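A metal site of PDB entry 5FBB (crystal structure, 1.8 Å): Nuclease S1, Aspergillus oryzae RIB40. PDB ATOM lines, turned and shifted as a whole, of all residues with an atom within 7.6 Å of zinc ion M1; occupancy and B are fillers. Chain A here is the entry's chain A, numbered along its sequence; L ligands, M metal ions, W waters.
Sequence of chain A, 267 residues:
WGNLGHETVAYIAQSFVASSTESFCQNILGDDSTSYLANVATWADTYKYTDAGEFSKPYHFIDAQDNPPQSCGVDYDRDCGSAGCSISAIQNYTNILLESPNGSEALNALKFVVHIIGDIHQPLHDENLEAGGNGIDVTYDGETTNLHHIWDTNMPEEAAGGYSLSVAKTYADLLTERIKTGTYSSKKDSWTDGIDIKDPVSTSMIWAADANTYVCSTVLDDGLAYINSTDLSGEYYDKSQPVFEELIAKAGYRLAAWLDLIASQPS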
ATOM      1  N   TRP A   1      12.435   6.265  12.034  1.00  0.00           N
ATOM      2  CA  TRP A   1      11.221   5.812  11.348  1.00  0.00           C
ATOM      3  C   TRP A   1      10.981   4.383  11.706  1.00  0.00           C
ATOM      4  O   TRP A   1      11.912   3.661  12.109  1.00  0.00           O
ATOM      5  CB  TRP A   1      11.380   5.895   9.785  1.00  0.00           C
ATOM      6  CG  TRP A   1      11.845   7.287   9.253  1.00  0.00           C
ATOM      7  CD1 TRP A   1      13.121   7.629   8.895  1.00  0.00           C
ATOM      8  CD2 TRP A   1      11.059   8.467   9.102  1.00  0.00           C
ATOM      9  NE1 TRP A   1      13.163   8.924   8.515  1.00  0.00           N
ATOM     10  CE2 TRP A   1      11.903   9.471   8.642  1.00  0.00           C
ATOM     11  CE3 TRP A   1       9.715   8.782   9.361  1.00  0.00           C
ATOM     12  CZ2 TRP A   1      11.476  10.761   8.383  1.00  0.00           C
ATOM     13  CZ3 TRP A   1       9.275  10.076   9.141  1.00  0.00           C
ATOM     14  CH2 TRP A   1      10.148  11.043   8.643  1.00  0.00           C
ATOM     15  N   GLY A   2       9.742   3.938  11.479  1.00  0.00           N
ATOM     16  CA  GLY A   2       9.416   2.544  11.527  1.00  0.00           C
ATOM     17  C   GLY A   2       9.762   1.900  10.207  1.00  0.00           C
ATOM     18  O   GLY A   2      10.426   2.516   9.325  1.00  0.00           O
ATOM     19  N   HIS A   6      11.902   3.380   6.656  1.00  0.00           N
ATOM     20  CA  HIS A   6      13.234   2.881   6.276  1.00  0.00           C
ATOM     21  C   HIS A   6      13.304   2.214   4.948  1.00  0.00           C
ATOM     22  O   HIS A   6      14.263   2.449   4.184  1.00  0.00           O
ATOM     23  CB  HIS A   6      13.800   1.966   7.339  1.00  0.00           C
ATOM     24  CG  HIS A   6      14.209   2.721   8.552  1.00  0.00           C
ATOM     25  ND1 HIS A   6      15.277   3.602   8.525  1.00  0.00           N
ATOM     26  CD2 HIS A   6      13.622   2.879   9.749  1.00  0.00           C
ATOM     27  CE1 HIS A   6      15.384   4.182   9.702  1.00  0.00           C
ATOM     28  NE2 HIS A   6      14.358   3.803  10.445  1.00  0.00           N
ATOM     29  N   ASP A  45      17.236  -1.918  13.521  1.00  0.00           N
ATOM     30  CA  ASP A  45      16.150  -1.865  14.500  1.00  0.00           C
ATOM     31  C   ASP A  45      15.940  -3.175  15.222  1.00  0.00           C
ATOM     32  O   ASP A  45      15.600  -3.160  16.395  1.00  0.00           O
ATOM     33  CB  ASP A  45      14.833  -1.334  13.966  1.00  0.00           C
ATOM     34  CG  ASP A  45      14.762   0.244  13.963  1.00  0.00           C
ATOM     35  OD1 ASP A  45      15.658   0.914  14.570  1.00  0.00           O
ATOM     36  OD2 ASP A  45      13.773   0.794  13.317  1.00  0.00           O
ATOM     37  N   LYS A  48      19.376  -3.674  17.671  1.00  0.00           N
ATOM     38  CA  LYS A  48      19.496  -2.897  18.871  1.00  0.00           C
ATOM     39  C   LYS A  48      18.731  -3.495  20.067  1.00  0.00           C
ATOM     40  O   LYS A  48      18.973  -3.058  21.225  1.00  0.00           O
ATOM     41  CB  LYS A  48      19.075  -1.446  18.655  1.00  0.00           C
ATOM     42  CG  LYS A  48      17.600  -1.234  18.582  1.00  0.00           C
ATOM     43  CD  LYS A  48      17.266   0.152  18.129  1.00  0.00           C
ATOM     44  CE  LYS A  48      15.802   0.481  18.198  1.00  0.00           C
ATOM     45  NZ  LYS A  48      15.602   1.868  17.722  1.00  0.00           N
ATOM     46  N   HIS A  60      20.892   5.490  16.684  1.00  0.00           N
ATOM     47  CA  HIS A  60      19.679   5.864  15.934  1.00  0.00           C
ATOM     48  C   HIS A  60      19.312   7.333  16.010  1.00  0.00           C
ATOM     49  O   HIS A  60      18.391   7.758  15.335  1.00  0.00           O
ATOM     50  CB  HIS A  60      18.491   4.949  16.301  1.00  0.00           C
ATOM     51  CG  HIS A  60      18.762   3.501  16.003  1.00  0.00           C
ATOM     52  ND1 HIS A  60      18.102   2.790  15.012  1.00  0.00           N
ATOM     53  CD2 HIS A  60      19.709   2.666  16.495  1.00  0.00           C
ATOM     54  CE1 HIS A  60      18.616   1.590  14.922  1.00  0.00           C
ATOM     55  NE2 HIS A  60      19.598   1.481  15.795  1.00  0.00           N
ATOM     56  N   PHE A  61      19.974   8.068  16.909  1.00  0.00           N
ATOM     57  CA  PHE A  61      19.552   9.412  17.168  1.00  0.00           C
ATOM     58  C   PHE A  61      20.683  10.275  17.697  1.00  0.00           C
ATOM     59  O   PHE A  61      21.760   9.827  18.000  1.00  0.00           O
ATOM     60  CB  PHE A  61      18.314   9.437  18.116  1.00  0.00           C
ATOM     61  CG  PHE A  61      18.582   8.758  19.411  1.00  0.00           C
ATOM     62  CD1 PHE A  61      19.210   9.430  20.465  1.00  0.00           C
ATOM     63  CD2 PHE A  61      18.211   7.436  19.601  1.00  0.00           C
ATOM     64  CE1 PHE A  61      19.489   8.761  21.663  1.00  0.00           C
ATOM     65  CE2 PHE A  61      18.544   6.759  20.763  1.00  0.00           C
ATOM     66  CZ  PHE A  61      19.172   7.411  21.792  1.00  0.00           C
ATOM     67  N   HIS A 115      20.234   2.444   7.239  1.00  0.00           N
ATOM     68  CA  HIS A 115      19.224   2.738   8.282  1.00  0.00           C
ATOM     69  C   HIS A 115      19.373   4.101   8.928  1.00  0.00           C
ATOM     70  O   HIS A 115      18.416   4.896   8.984  1.00  0.00           O
ATOM     71  CB  HIS A 115      19.251   1.640   9.329  1.00  0.00           C
ATOM     72  CG  HIS A 115      18.222   1.802  10.382  1.00  0.00           C
ATOM     73  ND1 HIS A 115      17.005   1.182  10.318  1.00  0.00           N
ATOM     74  CD2 HIS A 115      18.219   2.528  11.528  1.00  0.00           C
ATOM     75  CE1 HIS A 115      16.273   1.514  11.356  1.00  0.00           C
ATOM     76  NE2 HIS A 115      16.995   2.304  12.125  1.00  0.00           N
ATOM     77  N   ASP A 119      17.158   7.527   9.718  1.00  0.00           N
ATOM     78  CA  ASP A 119      16.822   8.032  11.072  1.00  0.00           C
ATOM     79  C   ASP A 119      17.206   9.486  11.314  1.00  0.00           C
ATOM     80  O   ASP A 119      16.436  10.215  11.939  1.00  0.00           O
ATOM     81  CB  ASP A 119      17.410   7.201  12.214  1.00  0.00           C
ATOM     82  CG  ASP A 119      16.572   6.007  12.577  1.00  0.00           C
ATOM     83  OD1 ASP A 119      15.348   5.956  12.193  1.00  0.00           O
ATOM     84  OD2 ASP A 119      17.126   5.074  13.235  1.00  0.00           O
ATOM     85  N   GLN A 122      14.362  11.852  10.480  1.00  0.00           N
ATOM     86  CA  GLN A 122      13.179  11.895  11.310  1.00  0.00           C
ATOM     87  C   GLN A 122      13.475  12.975  12.349  1.00  0.00           C
ATOM     88  O   GLN A 122      14.340  12.783  13.167  1.00  0.00           O
ATOM     89  CB  GLN A 122      12.902  10.526  11.909  1.00  0.00           C
ATOM     90  CG  GLN A 122      11.444  10.251  12.256  1.00  0.00           C
ATOM     91  CD  GLN A 122      10.904  10.976  13.495  1.00  0.00           C
ATOM     92  OE1 GLN A 122      10.929  12.198  13.590  1.00  0.00           O
ATOM     93  NE2 GLN A 122      10.361  10.184  14.452  1.00  0.00           N
ATOM     94  N   LEU A 124      12.372  14.018  15.146  1.00  0.00           N
ATOM     95  CA  LEU A 124      12.425  13.653  16.559  1.00  0.00           C
ATOM     96  C   LEU A 124      13.591  12.701  16.955  1.00  0.00           C
ATOM     97  O   LEU A 124      13.839  12.504  18.158  1.00  0.00           O
ATOM     98  CB  LEU A 124      11.085  13.119  17.017  1.00  0.00           C
ATOM     99  CG  LEU A 124       9.997  14.167  17.174  1.00  0.00           C
ATOM    100  CD1 LEU A 124       8.642  13.524  17.339  1.00  0.00           C
ATOM    101  CD2 LEU A 124      10.283  15.160  18.304  1.00  0.00           C
ATOM    102  N   HIS A 125      14.308  12.142  15.968  1.00  0.00           N
ATOM    103  CA  HIS A 125      15.581  11.487  16.181  1.00  0.00           C
ATOM    104  C   HIS A 125      16.740  12.498  16.317  1.00  0.00           C
ATOM    105  O   HIS A 125      17.923  12.104  16.441  1.00  0.00           O
ATOM    106  CB  HIS A 125      15.849  10.505  14.997  1.00  0.00           C
ATOM    107  CG  HIS A 125      15.111   9.204  15.136  1.00  0.00           C
ATOM    108  ND1 HIS A 125      15.749   8.007  15.326  1.00  0.00           N
ATOM    109  CD2 HIS A 125      13.778   8.935  15.152  1.00  0.00           C
ATOM    110  CE1 HIS A 125      14.863   7.044  15.454  1.00  0.00           C
ATOM    111  NE2 HIS A 125      13.644   7.579  15.357  1.00  0.00           N
ATOM    112  N   GLY A 132      13.081  12.122  22.546  1.00  0.00           N
ATOM    113  CA  GLY A 132      12.590  12.352  21.192  1.00  0.00           C
ATOM    114  C   GLY A 132      11.074  12.348  21.049  1.00  0.00           C
ATOM    115  O   GLY A 132      10.534  11.865  20.066  1.00  0.00           O
ATOM    116  N   ASN A 134       9.034  10.426  22.749  1.00  0.00           N
ATOM    117  CA  ASN A 134       8.441   9.154  23.193  1.00  0.00           C
ATOM    118  C   ASN A 134       7.595   9.336  24.472  1.00  0.00           C
ATOM    119  O   ASN A 134       6.592   8.644  24.696  1.00  0.00           O
ATOM    120  CB  ASN A 134       9.530   8.091  23.399  1.00  0.00           C
ATOM    121  CG  ASN A 134       9.930   7.414  22.104  1.00  0.00           C
ATOM    122  OD1 ASN A 134       9.165   6.640  21.570  1.00  0.00           O
ATOM    123  ND2 ASN A 134      11.150   7.638  21.644  1.00  0.00           N
ATOM    124  N   HIS A 148       6.414  10.598  19.223  1.00  0.00           N
ATOM    125  CA  HIS A 148       7.470   9.925  18.450  1.00  0.00           C
ATOM    126  C   HIS A 148       6.899   8.891  17.485  1.00  0.00           C
ATOM    127  O   HIS A 148       7.251   8.810  16.312  1.00  0.00           O
ATOM    128  CB  HIS A 148       8.468   9.271  19.382  1.00  0.00           C
ATOM    129  CG  HIS A 148       9.698   8.824  18.674  1.00  0.00           C
ATOM    130  ND1 HIS A 148      10.845   9.589  18.625  1.00  0.00           N
ATOM    131  CD2 HIS A 148       9.924   7.752  17.895  1.00  0.00           C
ATOM    132  CE1 HIS A 148      11.741   8.965  17.891  1.00  0.00           C
ATOM    133  NE2 HIS A 148      11.208   7.853  17.446  1.00  0.00           N
ATOM    134  N   HIS A 149       5.994   8.096  18.010  1.00  0.00           N
ATOM    135  CA  HIS A 149       5.369   6.983  17.276  1.00  0.00           C
ATOM    136  C   HIS A 149       4.557   7.436  16.062  1.00  0.00           C
ATOM    137  O   HIS A 149       4.614   6.784  14.981  1.00  0.00           O
ATOM    138  CB  HIS A 149       4.463   6.208  18.237  1.00  0.00           C
ATOM    139  CG  HIS A 149       4.038   4.858  17.728  1.00  0.00           C
ATOM    140  ND1 HIS A 149       2.953   4.684  16.918  1.00  0.00           N
ATOM    141  CD2 HIS A 149       4.497   3.620  18.036  1.00  0.00           C
ATOM    142  CE1 HIS A 149       2.779   3.382  16.693  1.00  0.00           C
ATOM    143  NE2 HIS A 149       3.711   2.714  17.342  1.00  0.00           N
ATOM    144  N   TRP A 151       5.118  10.136  14.234  1.00  0.00           N
ATOM    145  CA  TRP A 151       6.146  10.523  13.279  1.00  0.00           C
ATOM    146  C   TRP A 151       6.810   9.303  12.689  1.00  0.00           C
ATOM    147  O   TRP A 151       7.016   9.229  11.463  1.00  0.00           O
ATOM    148  CB  TRP A 151       7.167  11.517  13.864  1.00  0.00           C
ATOM    149  CG  TRP A 151       6.580  12.908  13.815  1.00  0.00           C
ATOM    150  CD1 TRP A 151       5.768  13.452  14.707  1.00  0.00           C
ATOM    151  CD2 TRP A 151       6.717  13.865  12.771  1.00  0.00           C
ATOM    152  NE1 TRP A 151       5.399  14.709  14.335  1.00  0.00           N
ATOM    153  CE2 TRP A 151       5.932  14.960  13.099  1.00  0.00           C
ATOM    154  CE3 TRP A 151       7.379  13.880  11.554  1.00  0.00           C
ATOM    155  CZ2 TRP A 151       5.864  16.103  12.309  1.00  0.00           C
ATOM    156  CZ3 TRP A 151       7.302  15.024  10.763  1.00  0.00           C
ATOM    157  CH2 TRP A 151       6.532  16.107  11.128  1.00  0.00           C
ATOM    158  N   ASP A 152       7.209   8.334  13.527  1.00  0.00           N
ATOM    159  CA  ASP A 152       7.849   7.119  12.977  1.00  0.00           C
ATOM    160  C   ASP A 152       6.965   6.283  12.044  1.00  0.00           C
ATOM    161  O   ASP A 152       7.458   5.705  11.049  1.00  0.00           O
ATOM    162  CB  ASP A 152       8.323   6.173  14.097  1.00  0.00           C
ATOM    163  CG  ASP A 152       9.790   6.480  14.613  1.00  0.00           C
ATOM    164  OD1 ASP A 152      10.544   7.326  14.041  1.00  0.00           O
ATOM    165  OD2 ASP A 152      10.170   5.770  15.557  1.00  0.00           O
ATOM    166  N   THR A 153       5.711   6.153  12.451  1.00  0.00           N
ATOM    167  CA  THR A 153       4.843   5.100  11.989  1.00  0.00           C
ATOM    168  C   THR A 153       3.471   5.582  11.542  1.00  0.00           C
ATOM    169  O   THR A 153       3.126   5.445  10.376  1.00  0.00           O
ATOM    170  CB  THR A 153       4.763   4.025  13.127  1.00  0.00           C
ATOM    171  OG1 THR A 153       6.060   3.413  13.254  1.00  0.00           O
ATOM    172  CG2 THR A 153       3.784   2.959  12.841  1.00  0.00           C
HETATM  173  P1  LIG L   1      13.626   3.797  14.966  1.00  0.00           P
HETATM  174  O1  LIG L   1      12.603   4.899  14.752  1.00  0.00           O
HETATM  175  O2  LIG L   1      14.616   3.833  16.140  1.00  0.00           O
HETATM  176  O3  LIG L   1      14.611   3.592  13.788  1.00  0.00           O
HETATM  177  O4  LIG L   1      12.714   2.533  15.168  1.00  0.00           O
HETATM  178  P1  LG2 L   2      17.614   8.937  27.687  1.00  0.00           P
HETATM  179  O1  LG2 L   2      18.252  10.001  26.734  1.00  0.00           O
HETATM  180  O2  LG2 L   2      18.561   7.788  27.986  1.00  0.00           O
HETATM  181  O3  LG2 L   2      16.946   9.482  28.966  1.00  0.00           O
HETATM  182  O4  LG2 L   2      16.505   8.244  26.759  1.00  0.00           O
HETATM  183  C1  LG2 L   2      15.726   7.144  27.253  1.00  0.00           C
HETATM  184  C2  LG2 L   2      15.414   6.189  26.130  1.00  0.00           C
HETATM  185  O5  LG2 L   2      14.859   6.885  24.980  1.00  0.00           O
HETATM  186  C3  LG2 L   2      16.596   5.367  25.623  1.00  0.00           C
HETATM  187  O6  LG2 L   2      16.220   4.010  25.424  1.00  0.00           O
HETATM  188  C4  LG2 L   2      16.948   6.032  24.296  1.00  0.00           C
HETATM  189  O7  LG2 L   2      17.370   5.044  23.375  1.00  0.00           O
HETATM  190  C5  LG2 L   2      15.622   6.615  23.819  1.00  0.00           C
HETATM  191  N1  LG2 L   2      15.777   7.875  23.078  1.00  0.00           N
HETATM  192  C6  LG2 L   2      16.382   9.013  23.540  1.00  0.00           C
HETATM  193  N2  LG2 L   2      16.404  10.002  22.678  1.00  0.00           N
HETATM  194  C7  LG2 L   2      15.749   9.466  21.569  1.00  0.00           C
HETATM  195  C8  LG2 L   2      15.440  10.015  20.313  1.00  0.00           C
HETATM  196  N3  LG2 L   2      15.664  11.276  19.986  1.00  0.00           N
HETATM  197  N4  LG2 L   2      14.812   9.217  19.394  1.00  0.00           N
HETATM  198  C9  LG2 L   2      14.511   7.951  19.770  1.00  0.00           C
HETATM  199  N5  LG2 L   2      14.720   7.353  20.952  1.00  0.00           N
HETATM  200  C10 LG2 L   2      15.355   8.162  21.805  1.00  0.00           C
HETATM  201 ZN    ZN M   1      12.041   6.399  16.089  1.00  0.00          ZN
HETATM  202 ZN    ZN M   2      13.769   4.655  12.240  1.00  0.00          ZN
HETATM  203 ZN    ZN M   3      16.433   3.253  13.870  1.00  0.00          ZN
HETATM  204  O   HOH W   1      12.761   5.299  17.694  1.00  0.00           O
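OD1 of Asp 152 lies close to N of Trp 1, 3.0 Å away. The side-chain carboxylate of Asp 152 lies within hydrogen-bond range of the side-chain amide nitrogen of Gln 122 (2.9 Å). The backbone carbonyl oxygen (O) of Asp 152 is in hydrogen-bond range of the backbone NH (N) of Gly 2, at 2.9 Å. The backbone carbonyl oxygen of His 60 sits at hydrogen-bond distance from a ring nitrogen (ND1) of His 125 (2.7 Å). The backbone carbonyl oxygen (O) of Gly 132 lies within hydrogen-bond range of a ring nitrogen (ND1) of His 148, 2.7 Å away.
Three residues have an atom within 4 Å of zinc ion M1: His 125, His 148 and Asp 152. The nearest printed residue that does not touch zinc ion M1 is Trp 1 (4.1 Å).
A nitrogen (N3) of LG2 L2 sits at hydrogen-bond distance from the backbone carbonyl oxygen (O) of Leu 124 (2.9 Å).
Zinc ion M1 is bound by the side-chain carboxylate of Asp 152 (2.0 Å), water W1 (2.1 Å), an oxygen (O1) of LIG L1 (2.1 Å), a ring nitrogen (NE2) of His 125 (2.1 Å) and a ring nitrogen (NE2) of His 148 (2.2 Å). Zinc ion M1 has five donor atoms within binding distance. Slightly farther from zinc ion M1 lies the side-chain carboxylate (OD1) of Asp 152 (2.7 Å).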
